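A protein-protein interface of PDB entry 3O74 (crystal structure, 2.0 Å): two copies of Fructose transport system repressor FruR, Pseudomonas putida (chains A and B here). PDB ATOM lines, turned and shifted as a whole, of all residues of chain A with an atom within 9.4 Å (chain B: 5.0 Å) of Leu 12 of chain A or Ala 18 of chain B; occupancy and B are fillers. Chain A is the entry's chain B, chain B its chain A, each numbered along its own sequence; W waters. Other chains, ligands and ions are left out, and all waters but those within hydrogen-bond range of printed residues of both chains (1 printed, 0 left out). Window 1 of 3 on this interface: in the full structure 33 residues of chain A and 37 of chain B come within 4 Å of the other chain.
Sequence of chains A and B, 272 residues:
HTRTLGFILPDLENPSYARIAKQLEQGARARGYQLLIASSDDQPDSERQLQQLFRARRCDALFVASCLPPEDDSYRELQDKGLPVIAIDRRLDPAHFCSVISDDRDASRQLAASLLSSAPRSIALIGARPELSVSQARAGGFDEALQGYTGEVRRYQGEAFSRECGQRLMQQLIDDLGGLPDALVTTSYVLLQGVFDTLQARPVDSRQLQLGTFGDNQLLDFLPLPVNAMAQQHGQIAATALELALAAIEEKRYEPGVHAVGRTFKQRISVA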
ATOM      1  N   PHE A   7      -4.207 -15.611  12.975  1.00  0.00           N
ATOM      2  CA  PHE A   7      -5.078 -16.738  12.691  1.00  0.00           C
ATOM      3  C   PHE A   7      -4.312 -17.801  11.906  1.00  0.00           C
ATOM      4  O   PHE A   7      -3.908 -17.575  10.767  1.00  0.00           O
ATOM      5  CB  PHE A   7      -6.321 -16.284  11.915  1.00  0.00           C
ATOM      6  CG  PHE A   7      -7.362 -17.367  11.727  1.00  0.00           C
ATOM      7  CD1 PHE A   7      -7.338 -18.527  12.491  1.00  0.00           C
ATOM      8  CD2 PHE A   7      -8.378 -17.210  10.793  1.00  0.00           C
ATOM      9  CE1 PHE A   7      -8.301 -19.521  12.316  1.00  0.00           C
ATOM     10  CE2 PHE A   7      -9.340 -18.192  10.617  1.00  0.00           C
ATOM     11  CZ  PHE A   7      -9.305 -19.349  11.381  1.00  0.00           C
ATOM     12  N   ILE A   8      -4.094 -18.950  12.534  1.00  0.00           N
ATOM     13  CA  ILE A   8      -3.485 -20.086  11.862  1.00  0.00           C
ATOM     14  C   ILE A   8      -4.587 -21.020  11.395  1.00  0.00           C
ATOM     15  O   ILE A   8      -5.325 -21.576  12.214  1.00  0.00           O
ATOM     16  CB  ILE A   8      -2.567 -20.871  12.810  1.00  0.00           C
ATOM     17  CG1 ILE A   8      -1.375 -20.017  13.235  1.00  0.00           C
ATOM     18  CG2 ILE A   8      -2.093 -22.156  12.146  1.00  0.00           C
ATOM     19  CD1 ILE A   8      -0.470 -20.703  14.241  1.00  0.00           C
ATOM     20  N   LEU A   9      -4.702 -21.199  10.083  1.00  0.00           N
ATOM     21  CA  LEU A   9      -5.703 -22.105   9.537  1.00  0.00           C
ATOM     22  C   LEU A   9      -5.046 -23.169   8.651  1.00  0.00           C
ATOM     23  O   LEU A   9      -3.914 -22.992   8.194  1.00  0.00           O
ATOM     24  CB  LEU A   9      -6.793 -21.321   8.802  1.00  0.00           C
ATOM     25  CG  LEU A   9      -6.345 -20.312   7.747  1.00  0.00           C
ATOM     26  CD1 LEU A   9      -6.007 -21.019   6.444  1.00  0.00           C
ATOM     27  CD2 LEU A   9      -7.416 -19.262   7.515  1.00  0.00           C
ATOM     28  N   PRO A  10      -5.745 -24.291   8.431  1.00  0.00           N
ATOM     29  CA  PRO A  10      -5.126 -25.422   7.733  1.00  0.00           C
ATOM     30  C   PRO A  10      -5.036 -25.244   6.224  1.00  0.00           C
ATOM     31  O   PRO A  10      -4.120 -25.781   5.610  1.00  0.00           O
ATOM     32  CB  PRO A  10      -6.072 -26.587   8.046  1.00  0.00           C
ATOM     33  CG  PRO A  10      -6.926 -26.123   9.172  1.00  0.00           C
ATOM     34  CD  PRO A  10      -7.057 -24.651   8.987  1.00  0.00           C
ATOM     35  N   ASP A  11      -5.972 -24.512   5.635  1.00  0.00           N
ATOM     36  CA  ASP A  11      -6.081 -24.481   4.182  1.00  0.00           C
ATOM     37  C   ASP A  11      -6.757 -23.215   3.684  1.00  0.00           C
ATOM     38  O   ASP A  11      -7.950 -23.000   3.895  1.00  0.00           O
ATOM     39  CB  ASP A  11      -6.846 -25.713   3.694  1.00  0.00           C
ATOM     40  CG  ASP A  11      -6.866 -25.834   2.179  1.00  0.00           C
ATOM     41  OD1 ASP A  11      -6.325 -24.943   1.488  1.00  0.00           O
ATOM     42  OD2 ASP A  11      -7.428 -26.830   1.678  1.00  0.00           O
ATOM     43  N   LEU A  12      -5.975 -22.385   3.005  1.00  0.00           N
ATOM     44  CA  LEU A  12      -6.468 -21.129   2.458  1.00  0.00           C
ATOM     45  C   LEU A  12      -7.553 -21.347   1.410  1.00  0.00           C
ATOM     46  O   LEU A  12      -8.387 -20.472   1.180  1.00  0.00           O
ATOM     47  CB  LEU A  12      -5.313 -20.345   1.838  1.00  0.00           C
ATOM     48  CG  LEU A  12      -4.297 -19.774   2.826  1.00  0.00           C
ATOM     49  CD1 LEU A  12      -3.028 -19.335   2.111  1.00  0.00           C
ATOM     50  CD2 LEU A  12      -4.919 -18.618   3.590  1.00  0.00           C
ATOM     51  N   GLU A  13      -7.533 -22.513   0.770  1.00  0.00           N
ATOM     52  CA  GLU A  13      -8.485 -22.799  -0.301  1.00  0.00           C
ATOM     53  C   GLU A  13      -9.826 -23.335   0.207  1.00  0.00           C
ATOM     54  O   GLU A  13     -10.794 -23.412  -0.550  1.00  0.00           O
ATOM     55  CB  GLU A  13      -7.875 -23.752  -1.332  1.00  0.00           C
ATOM     56  CG  GLU A  13      -6.804 -23.121  -2.199  1.00  0.00           C
ATOM     57  CD  GLU A  13      -6.214 -24.099  -3.198  1.00  0.00           C
ATOM     58  OE1 GLU A  13      -6.418 -25.322  -3.037  1.00  0.00           O
ATOM     59  OE2 GLU A  13      -5.544 -23.639  -4.143  1.00  0.00           O
ATOM     60  N   ASN A  14      -9.878 -23.716   1.479  1.00  0.00           N
ATOM     61  CA  ASN A  14     -11.138 -24.112   2.099  1.00  0.00           C
ATOM     62  C   ASN A  14     -12.007 -22.877   2.326  1.00  0.00           C
ATOM     63  O   ASN A  14     -11.662 -22.013   3.131  1.00  0.00           O
ATOM     64  CB  ASN A  14     -10.875 -24.841   3.417  1.00  0.00           C
ATOM     65  CG  ASN A  14     -12.141 -25.399   4.040  1.00  0.00           C
ATOM     66  OD1 ASN A  14     -13.245 -24.931   3.763  1.00  0.00           O
ATOM     67  ND2 ASN A  14     -11.985 -26.403   4.895  1.00  0.00           N
ATOM     68  N   PRO A  15     -13.137 -22.788   1.607  1.00  0.00           N
ATOM     69  CA  PRO A  15     -13.992 -21.596   1.609  1.00  0.00           C
ATOM     70  C   PRO A  15     -14.544 -21.244   2.988  1.00  0.00           C
ATOM     71  O   PRO A  15     -14.825 -20.075   3.250  1.00  0.00           O
ATOM     72  CB  PRO A  15     -15.139 -21.988   0.671  1.00  0.00           C
ATOM     73  CG  PRO A  15     -14.578 -23.055  -0.192  1.00  0.00           C
ATOM     74  CD  PRO A  15     -13.637 -23.821   0.685  1.00  0.00           C
ATOM     75  N   SER A  16     -14.702 -22.241   3.853  1.00  0.00           N
ATOM     76  CA  SER A  16     -15.205 -21.994   5.200  1.00  0.00           C
ATOM     77  C   SER A  16     -14.181 -21.251   6.051  1.00  0.00           C
ATOM     78  O   SER A  16     -14.524 -20.321   6.780  1.00  0.00           O
ATOM     79  CB  SER A  16     -15.608 -23.306   5.875  1.00  0.00           C
ATOM     80  OG  SER A  16     -16.697 -23.901   5.198  1.00  0.00           O
ATOM     81  N   TYR A  17     -12.920 -21.658   5.957  1.00  0.00           N
ATOM     82  CA  TYR A  17     -11.871 -20.953   6.677  1.00  0.00           C
ATOM     83  C   TYR A  17     -11.697 -19.529   6.146  1.00  0.00           C
ATOM     84  O   TYR A  17     -11.490 -18.598   6.919  1.00  0.00           O
ATOM     85  CB  TYR A  17     -10.558 -21.736   6.643  1.00  0.00           C
ATOM     86  CG  TYR A  17     -10.581 -22.964   7.526  1.00  0.00           C
ATOM     87  CD1 TYR A  17     -10.839 -22.857   8.887  1.00  0.00           C
ATOM     88  CD2 TYR A  17     -10.341 -24.229   7.003  1.00  0.00           C
ATOM     89  CE1 TYR A  17     -10.860 -23.980   9.705  1.00  0.00           C
ATOM     90  CE2 TYR A  17     -10.361 -25.356   7.815  1.00  0.00           C
ATOM     91  CZ  TYR A  17     -10.622 -25.224   9.162  1.00  0.00           C
ATOM     92  OH  TYR A  17     -10.643 -26.338   9.973  1.00  0.00           O
ATOM     93  N   ALA A  18     -11.799 -19.364   4.829  1.00  0.00           N
ATOM     94  CA  ALA A  18     -11.701 -18.040   4.215  1.00  0.00           C
ATOM     95  C   ALA A  18     -12.830 -17.126   4.693  1.00  0.00           C
ATOM     96  O   ALA A  18     -12.605 -15.960   5.027  1.00  0.00           O
ATOM     97  CB  ALA A  18     -11.710 -18.154   2.692  1.00  0.00           C
ATOM     98  N   ARG A  19     -14.043 -17.665   4.726  1.00  0.00           N
ATOM     99  CA  ARG A  19     -15.199 -16.913   5.186  1.00  0.00           C
ATOM    100  C   ARG A  19     -15.040 -16.502   6.648  1.00  0.00           C
ATOM    101  O   ARG A  19     -15.265 -15.345   7.011  1.00  0.00           O
ATOM    102  CB  ARG A  19     -16.474 -17.734   5.007  1.00  0.00           C
ATOM    103  CG  ARG A  19     -17.690 -17.109   5.661  1.00  0.00           C
ATOM    104  CD  ARG A  19     -18.327 -16.048   4.787  1.00  0.00           C
ATOM    105  NE  ARG A  19     -18.965 -16.637   3.616  1.00  0.00           N
ATOM    106  CZ  ARG A  19     -20.214 -16.380   3.238  1.00  0.00           C
ATOM    107  NH1 ARG A  19     -20.959 -15.535   3.937  1.00  0.00           N
ATOM    108  NH2 ARG A  19     -20.712 -16.965   2.157  1.00  0.00           N
ATOM    109  N   ILE A  20     -14.636 -17.448   7.486  1.00  0.00           N
ATOM    110  CA  ILE A  20     -14.399 -17.152   8.890  1.00  0.00           C
ATOM    111  C   ILE A  20     -13.286 -16.116   9.040  1.00  0.00           C
ATOM    112  O   ILE A  20     -13.426 -15.147   9.783  1.00  0.00           O
ATOM    113  CB  ILE A  20     -14.050 -18.427   9.685  1.00  0.00           C
ATOM    114  CG1 ILE A  20     -15.276 -19.342   9.784  1.00  0.00           C
ATOM    115  CG2 ILE A  20     -13.542 -18.064  11.071  1.00  0.00           C
ATOM    116  CD1 ILE A  20     -14.978 -20.713  10.377  1.00  0.00           C
ATOM    117  N   ALA A  21     -12.186 -16.317   8.321  1.00  0.00           N
ATOM    118  CA  ALA A  21     -11.068 -15.377   8.362  1.00  0.00           C
ATOM    119  C   ALA A  21     -11.508 -13.975   7.951  1.00  0.00           C
ATOM    120  O   ALA A  21     -11.053 -12.982   8.516  1.00  0.00           O
ATOM    121  CB  ALA A  21      -9.929 -15.863   7.474  1.00  0.00           C
ATOM    122  N   LEU A  36      -3.727 -10.931  11.049  1.00  0.00           N
ATOM    123  CA  LEU A  36      -2.721 -11.554  10.202  1.00  0.00           C
ATOM    124  C   LEU A  36      -3.023 -13.038  10.073  1.00  0.00           C
ATOM    125  O   LEU A  36      -3.196 -13.744  11.069  1.00  0.00           O
ATOM    126  CB  LEU A  36      -1.317 -11.339  10.757  1.00  0.00           C
ATOM    127  CG  LEU A  36      -0.821  -9.892  10.797  1.00  0.00           C
ATOM    128  CD1 LEU A  36       0.523  -9.814  11.505  1.00  0.00           C
ATOM    129  CD2 LEU A  36      -0.731  -9.309   9.394  1.00  0.00           C
ATOM    130  N   ILE A  37      -3.089 -13.503   8.833  1.00  0.00           N
ATOM    131  CA  ILE A  37      -3.467 -14.875   8.549  1.00  0.00           C
ATOM    132  C   ILE A  37      -2.271 -15.671   8.035  1.00  0.00           C
ATOM    133  O   ILE A  37      -1.444 -15.163   7.270  1.00  0.00           O
ATOM    134  CB  ILE A  37      -4.615 -14.913   7.528  1.00  0.00           C
ATOM    135  CG1 ILE A  37      -5.839 -14.201   8.104  1.00  0.00           C
ATOM    136  CG2 ILE A  37      -4.938 -16.340   7.132  1.00  0.00           C
ATOM    137  CD1 ILE A  37      -6.894 -13.859   7.071  1.00  0.00           C
ATOM    138  N   ALA A  38      -2.179 -16.920   8.474  1.00  0.00           N
ATOM    139  CA  ALA A  38      -1.129 -17.812   8.014  1.00  0.00           C
ATOM    140  C   ALA A  38      -1.702 -19.211   7.869  1.00  0.00           C
ATOM    141  O   ALA A  38      -2.621 -19.592   8.600  1.00  0.00           O
ATOM    142  CB  ALA A  38       0.033 -17.807   8.979  1.00  0.00           C
ATOM    143  N   SER A  39      -1.160 -19.972   6.922  1.00  0.00           N
ATOM    144  CA  SER A  39      -1.665 -21.312   6.651  1.00  0.00           C
ATOM    145  C   SER A  39      -0.627 -22.384   6.966  1.00  0.00           C
ATOM    146  O   SER A  39       0.523 -22.299   6.529  1.00  0.00           O
ATOM    147  CB  SER A  39      -2.121 -21.434   5.197  1.00  0.00           C
ATOM    148  OG  SER A  39      -2.412 -22.784   4.884  1.00  0.00           O
ATOM    149  N   SER A  40      -1.049 -23.390   7.728  1.00  0.00           N
ATOM    150  CA  SER A  40      -0.196 -24.508   8.108  1.00  0.00           C
ATOM    151  C   SER A  40      -0.196 -25.578   7.024  1.00  0.00           C
ATOM    152  O   SER A  40       0.663 -26.461   7.006  1.00  0.00           O
ATOM    153  CB  SER A  40      -0.718 -25.138   9.396  1.00  0.00           C
ATOM    154  OG  SER A  40      -1.949 -25.795   9.147  1.00  0.00           O
ATOM    155  N   ASP A  41      -1.179 -25.511   6.134  1.00  0.00           N
ATOM    156  CA  ASP A  41      -1.369 -26.550   5.133  1.00  0.00           C
ATOM    157  C   ASP A  41      -1.636 -27.897   5.805  1.00  0.00           C
ATOM    158  O   ASP A  41      -1.350 -28.949   5.237  1.00  0.00           O
ATOM    159  CB  ASP A  41      -0.151 -26.646   4.217  1.00  0.00           C
ATOM    160  CG  ASP A  41      -0.524 -26.588   2.755  1.00  0.00           C
ATOM    161  OD1 ASP A  41      -0.862 -27.646   2.189  1.00  0.00           O
ATOM    162  OD2 ASP A  41      -0.488 -25.482   2.173  1.00  0.00           O
ATOM    163  N   ASP A  42      -2.181 -27.853   7.018  1.00  0.00           N
ATOM    164  CA  ASP A  42      -2.476 -29.062   7.784  1.00  0.00           C
ATOM    165  C   ASP A  42      -1.229 -29.907   8.068  1.00  0.00           C
ATOM    166  O   ASP A  42      -1.333 -31.096   8.364  1.00  0.00           O
ATOM    167  CB  ASP A  42      -3.557 -29.903   7.090  1.00  0.00           C
ATOM    168  CG  ASP A  42      -4.788 -30.110   7.965  1.00  0.00           C
ATOM    169  OD1 ASP A  42      -4.681 -29.923   9.194  1.00  0.00           O
ATOM    170  OD2 ASP A  42      -5.860 -30.460   7.431  1.00  0.00           O
ATOM    171  N   LEU A  50       4.725 -21.533  12.435  1.00  0.00           N
ATOM    172  CA  LEU A  50       3.845 -20.373  12.533  1.00  0.00           C
ATOM    173  C   LEU A  50       3.649 -19.944  13.983  1.00  0.00           C
ATOM    174  O   LEU A  50       3.489 -18.758  14.272  1.00  0.00           O
ATOM    175  CB  LEU A  50       2.497 -20.652  11.863  1.00  0.00           C
ATOM    176  CG  LEU A  50       2.572 -20.839  10.345  1.00  0.00           C
ATOM    177  CD1 LEU A  50       1.196 -21.107   9.766  1.00  0.00           C
ATOM    178  CD2 LEU A  50       3.191 -19.617   9.703  1.00  0.00           C
ATOM    179  N   PHE A 161      -7.697 -33.781   4.132  1.00  0.00           N
ATOM    180  CA  PHE A 161      -8.892 -33.151   3.592  1.00  0.00           C
ATOM    181  C   PHE A 161      -8.546 -32.532   2.243  1.00  0.00           C
ATOM    182  O   PHE A 161      -8.314 -31.328   2.140  1.00  0.00           O
ATOM    183  CB  PHE A 161      -9.431 -32.087   4.543  1.00  0.00           C
ATOM    184  CG  PHE A 161      -9.994 -32.644   5.826  1.00  0.00           C
ATOM    185  CD1 PHE A 161     -11.204 -33.323   5.831  1.00  0.00           C
ATOM    186  CD2 PHE A 161      -9.322 -32.473   7.026  1.00  0.00           C
ATOM    187  CE1 PHE A 161     -11.730 -33.830   7.010  1.00  0.00           C
ATOM    188  CE2 PHE A 161      -9.841 -32.974   8.208  1.00  0.00           C
ATOM    189  CZ  PHE A 161     -11.047 -33.654   8.201  1.00  0.00           C
ATOM    190  N   LEU B  12     -10.426 -12.450   0.609  1.00  0.00           N
ATOM    191  CA  LEU B  12     -10.048 -13.803   1.005  1.00  0.00           C
ATOM    192  C   LEU B  12     -10.972 -14.851   0.385  1.00  0.00           C
ATOM    193  O   LEU B  12     -10.566 -15.989   0.141  1.00  0.00           O
ATOM    194  CB  LEU B  12     -10.077 -13.920   2.530  1.00  0.00           C
ATOM    195  CG  LEU B  12      -9.042 -13.080   3.284  1.00  0.00           C
ATOM    196  CD1 LEU B  12      -9.552 -12.651   4.656  1.00  0.00           C
ATOM    197  CD2 LEU B  12      -7.734 -13.846   3.399  1.00  0.00           C
ATOM    198  N   ASN B  14     -12.333 -14.617  -2.563  1.00  0.00           N
ATOM    199  CA  ASN B  14     -12.107 -14.734  -4.002  1.00  0.00           C
ATOM    200  C   ASN B  14     -11.122 -15.866  -4.268  1.00  0.00           C
ATOM    201  O   ASN B  14      -9.953 -15.765  -3.904  1.00  0.00           O
ATOM    202  CB  ASN B  14     -11.596 -13.414  -4.588  1.00  0.00           C
ATOM    203  CG  ASN B  14     -11.504 -13.445  -6.110  1.00  0.00           C
ATOM    204  OD1 ASN B  14     -11.086 -14.443  -6.699  1.00  0.00           O
ATOM    205  ND2 ASN B  14     -11.893 -12.348  -6.748  1.00  0.00           N
ATOM    206  N   PRO B  15     -11.594 -16.951  -4.904  1.00  0.00           N
ATOM    207  CA  PRO B  15     -10.784 -18.157  -5.122  1.00  0.00           C
ATOM    208  C   PRO B  15      -9.466 -17.892  -5.846  1.00  0.00           C
ATOM    209  O   PRO B  15      -8.506 -18.636  -5.642  1.00  0.00           O
ATOM    210  CB  PRO B  15     -11.693 -19.035  -5.987  1.00  0.00           C
ATOM    211  CG  PRO B  15     -13.072 -18.597  -5.642  1.00  0.00           C
ATOM    212  CD  PRO B  15     -12.977 -17.119  -5.386  1.00  0.00           C
ATOM    213  N   SER B  16      -9.418 -16.858  -6.679  1.00  0.00           N
ATOM    214  CA  SER B  16      -8.193 -16.529  -7.398  1.00  0.00           C
ATOM    215  C   SER B  16      -7.097 -16.068  -6.449  1.00  0.00           C
ATOM    216  O   SER B  16      -5.949 -16.494  -6.558  1.00  0.00           O
ATOM    217  CB  SER B  16      -8.451 -15.454  -8.456  1.00  0.00           C
ATOM    218  OG  SER B  16      -8.910 -16.034  -9.662  1.00  0.00           O
ATOM    219  N   TYR B  17      -7.458 -15.195  -5.518  1.00  0.00           N
ATOM    220  CA  TYR B  17      -6.492 -14.686  -4.555  1.00  0.00           C
ATOM    221  C   TYR B  17      -6.086 -15.754  -3.551  1.00  0.00           C
ATOM    222  O   TYR B  17      -4.915 -15.856  -3.189  1.00  0.00           O
ATOM    223  CB  TYR B  17      -7.046 -13.454  -3.841  1.00  0.00           C
ATOM    224  CG  TYR B  17      -7.121 -12.255  -4.744  1.00  0.00           C
ATOM    225  CD1 TYR B  17      -8.332 -11.629  -5.009  1.00  0.00           C
ATOM    226  CD2 TYR B  17      -5.979 -11.762  -5.356  1.00  0.00           C
ATOM    227  CE1 TYR B  17      -8.396 -10.529  -5.847  1.00  0.00           C
ATOM    228  CE2 TYR B  17      -6.032 -10.670  -6.196  1.00  0.00           C
ATOM    229  CZ  TYR B  17      -7.243 -10.058  -6.440  1.00  0.00           C
ATOM    230  OH  TYR B  17      -7.290  -8.970  -7.275  1.00  0.00           O
ATOM    231  N   ALA B  18      -7.051 -16.553  -3.115  1.00  0.00           N
ATOM    232  CA  ALA B  18      -6.770 -17.634  -2.174  1.00  0.00           C
ATOM    233  C   ALA B  18      -5.774 -18.620  -2.779  1.00  0.00           C
ATOM    234  O   ALA B  18      -4.864 -19.099  -2.103  1.00  0.00           O
ATOM    235  CB  ALA B  18      -8.056 -18.345  -1.775  1.00  0.00           C
ATOM    236  N   ARG B  19      -5.949 -18.909  -4.064  1.00  0.00           N
ATOM    237  CA  ARG B  19      -5.072 -19.826  -4.774  1.00  0.00           C
ATOM    238  C   ARG B  19      -3.648 -19.292  -4.873  1.00  0.00           C
ATOM    239  O   ARG B  19      -2.693 -19.999  -4.566  1.00  0.00           O
ATOM    240  CB  ARG B  19      -5.624 -20.089  -6.171  1.00  0.00           C
ATOM    241  CG  ARG B  19      -6.551 -21.274  -6.257  1.00  0.00           C
ATOM    242  CD  ARG B  19      -5.804 -22.463  -6.812  1.00  0.00           C
ATOM    243  NE  ARG B  19      -6.696 -23.564  -7.155  1.00  0.00           N
ATOM    244  CZ  ARG B  19      -6.360 -24.564  -7.960  1.00  0.00           C
ATOM    245  NH1 ARG B  19      -5.153 -24.596  -8.511  1.00  0.00           N
ATOM    246  NH2 ARG B  19      -7.231 -25.528  -8.223  1.00  0.00           N
ATOM    247  N   ILE B  20      -3.513 -18.042  -5.305  1.00  0.00           N
ATOM    248  CA  ILE B  20      -2.207 -17.405  -5.407  1.00  0.00           C
ATOM    249  C   ILE B  20      -1.535 -17.302  -4.044  1.00  0.00           C
ATOM    250  O   ILE B  20      -0.329 -17.510  -3.923  1.00  0.00           O
ATOM    251  CB  ILE B  20      -2.306 -15.990  -6.010  1.00  0.00           C
ATOM    252  CG1 ILE B  20      -2.815 -16.057  -7.451  1.00  0.00           C
ATOM    253  CG2 ILE B  20      -0.949 -15.298  -5.970  1.00  0.00           C
ATOM    254  CD1 ILE B  20      -2.941 -14.705  -8.113  1.00  0.00           C
ATOM    255  N   ALA B  21      -2.316 -16.975  -3.020  1.00  0.00           N
ATOM    256  CA  ALA B  21      -1.774 -16.879  -1.667  1.00  0.00           C
ATOM    257  C   ALA B  21      -1.246 -18.229  -1.206  1.00  0.00           C
ATOM    258  O   ALA B  21      -0.152 -18.327  -0.651  1.00  0.00           O
ATOM    259  CB  ALA B  21      -2.829 -16.360  -0.700  1.00  0.00           C
ATOM    260  N   LYS B  22      -2.003 -19.266  -1.431  1.00  0.00           N
ATOM    261  CA  LYS B  22      -1.624 -20.607  -1.091  1.00  0.00           C
ATOM    262  C   LYS B  22      -0.354 -21.036  -1.803  1.00  0.00           C
ATOM    263  O   LYS B  22       0.515 -21.599  -1.231  1.00  0.00           O
ATOM    264  CB  LYS B  22      -2.746 -21.584  -1.378  1.00  0.00           C
ATOM    265  CG  LYS B  22      -2.414 -23.011  -1.082  1.00  0.00           C
ATOM    266  CD  LYS B  22      -3.644 -23.846  -0.908  1.00  0.00           C
ATOM    267  CE  LYS B  22      -3.393 -25.183  -0.278  1.00  0.00           C
ATOM    268  NZ  LYS B  22      -4.469 -26.177  -0.529  1.00  0.00           N
ATOM    269  N   GLN B  23      -0.261 -20.730  -3.064  1.00  0.00           N
ATOM    270  CA  GLN B  23       0.927 -21.065  -3.845  1.00  0.00           C
ATOM    271  C   GLN B  23       2.143 -20.275  -3.374  1.00  0.00           C
ATOM    272  O   GLN B  23       3.253 -20.797  -3.312  1.00  0.00           O
ATOM    273  CB  GLN B  23       0.678 -20.795  -5.332  1.00  0.00           C
ATOM    274  CG  GLN B  23       0.996 -21.969  -6.236  1.00  0.00           C
ATOM    275  CD  GLN B  23       0.006 -23.105  -6.079  1.00  0.00           C
ATOM    276  OE1 GLN B  23       0.259 -24.227  -6.516  1.00  0.00           O
ATOM    277  NE2 GLN B  23      -1.131 -22.820  -5.454  1.00  0.00           N
ATOM    278  N   GLU B  25       2.556 -19.034  -0.344  1.00  0.00           N
ATOM    279  CA  GLU B  25       2.912 -19.586   0.954  1.00  0.00           C
ATOM    280  C   GLU B  25       3.794 -20.818   0.785  1.00  0.00           C
ATOM    281  O   GLU B  25       4.866 -20.907   1.380  1.00  0.00           O
ATOM    282  CB  GLU B  25       1.647 -19.923   1.750  1.00  0.00           C
ATOM    283  CG  GLU B  25       1.849 -20.927   2.867  1.00  0.00           C
ATOM    284  CD  GLU B  25       0.886 -22.097   2.765  1.00  0.00           C
ATOM    285  OE1 GLU B  25       1.124 -23.128   3.428  1.00  0.00           O
ATOM    286  OE2 GLU B  25      -0.106 -21.990   2.014  1.00  0.00           O
ATOM    287  N   ILE B  37      -0.614 -13.049   5.602  1.00  0.00           N
ATOM    288  CA  ILE B  37      -1.637 -12.580   4.683  1.00  0.00           C
ATOM    289  C   ILE B  37      -2.629 -11.657   5.382  1.00  0.00           C
ATOM    290  O   ILE B  37      -3.039 -11.911   6.510  1.00  0.00           O
ATOM    291  CB  ILE B  37      -2.410 -13.771   4.111  1.00  0.00           C
ATOM    292  CG1 ILE B  37      -1.458 -14.707   3.365  1.00  0.00           C
ATOM    293  CG2 ILE B  37      -3.535 -13.301   3.210  1.00  0.00           C
ATOM    294  CD1 ILE B  37      -1.988 -16.120   3.219  1.00  0.00           C
HETATM  295  O   HOH W   1     -10.941 -18.985  -0.382  1.00  0.00           O
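CB of Ala 18 of chain B touches O of Leu 12 of chain A, at 3.7 Å.
Leu 12 of chain A touches Ala 21 of chain B (CD1 to C, 3.9 Å).
N of Lys 22 of chain B touches CD1 of Leu 12 of chain A, 3.7 Å away.
CD1 of Leu 12 of chain A touches CD1 of Ile 37 of chain B (3.6 Å).
Ala 18 of chain A touches Leu 12 of chain B.
O of Ile 37 of chain B touches CA of Leu 36 of chain A, at 3.7 Å.
CE of Lys 22 of chain B touches OD2 of Asp 41 of chain A (3.8 Å).
Leu 12 of chain A touches Ala 18 of chain B, and with the chains exchanged Ala 18 of chain A touches Leu 12 of chain B.
Leu 12 of chain A touches Ala 21 of chain B, but with the chains exchanged Ala 21 of chain A does not touch Leu 12 of chain B (4.1 Å).
Leu 12 of chain A touches Ile 37 of chain B, and with the chains exchanged Ile 37 of chain A touches Leu 12 of chain B.
Ile 37 of chain B touches its own counterpart, Ile 37 of chain A.
Water W1 bridges the backbone carbonyl oxygen of Leu 12 of chain B (3.1 Å) and the backbone carbonyl oxygen of Leu 12 of chain A (3.3 Å).
Printed residues of chain A that touch a printed residue of chain B: Asp 11, Leu 12, Glu 13, Ala 18, Leu 36, Ile 37, Ser 39 and Asp 41.
Hydrophobic or aromatic side chains of chain A that line the printed part of chain B: Leu 12, Ala 18 and Ile 37.
Among the printed residues, 15 pairs touch across the chains.
Among the printed residues, Asp or Glu carboxylates within 4 Å of a Lys or Arg side-chain nitrogen of the other chain: Asp 11 of chain A with Lys 22 of chain B (3.0 Å), Glu 13 of chain A with Arg 19 of chain B (3.2 Å) and Glu 13 of chain A with Lys 22 of chain B (3.3 Å).
The side-chain carboxylate (OE2) of Glu 13 of chain A is in salt-bridge range of the guanidinium group (NE) of Arg 19 of chain B, 3.2 Å away.
NZ of Lys 22 of chain B is in salt-bridge range of OD1 of Asp 11 of chain A.
NZ of Lys 22 of chain B is in salt-bridge range of OE1 of Glu 13 of chain A, at 3.3 Å.
O of Ile 37 of chain B is in hydrogen-bond range of N of Ile 37 of chain A (2.8 Å).
The backbone carbonyl oxygen (O) of Ser 39 of chain A sits close to the side-chain carboxylate (OE1) of Glu 25 of chain B (3.3 Å).
OD2 of Asp 41 of chain A sits close to OE1 of Glu 25 of chain B (3.1 Å).
The side-chain amide nitrogen of Gln 23 of chain B lies within hydrogen-bond range of the backbone carbonyl oxygen of Arg 19 of chain B, at 3.3 Å.
The backbone carbonyl oxygen of Leu 36 of chain A lies within hydrogen-bond range of the backbone NH of Phe 7 of chain A, 2.9 Å away.
OG of Ser 39 of chain A sits at hydrogen-bond distance from N of Asp 41 of chain A (3.2 Å).
Leu 12 of chain A touches just these residues of chain B: Ala 18, Ala 21, Lys 22, Glu 25 and Ile 37.
Printed residues of chain B within 4 Å of Leu 36 of chain A: Ile 37 (3.7 Å).
Printed residues of chain B within 4 Å of Ile 37 of chain A: Leu 12 (3.8 Å) and Ile 37 (2.8 Å).
Leu 50 of chain A touches none of the printed residues of chain B.
Ala 18 of chain B touches just one residue of chain A: Leu 12.
Of the printed residues of chain A, Arg 19 of chain B touches Glu 13.
Of chain A, only Leu 12 comes within 4 Å of Ala 21 of chain B.
Printed residues of chain A within 4 Å of Lys 22 of chain B: Asp 11 (3.0 Å), Leu 12 (3.7 Å), Glu 13 (3.3 Å) and Asp 41 (3.8 Å).
The nearest residue of chain A that does not touch Ala 18 of chain B is Glu 13 of chain A (4.5 Å).
The nearest printed residue of chain A that does not touch Glu 25 of chain B is Ser 40 of chain A (4.5 Å).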
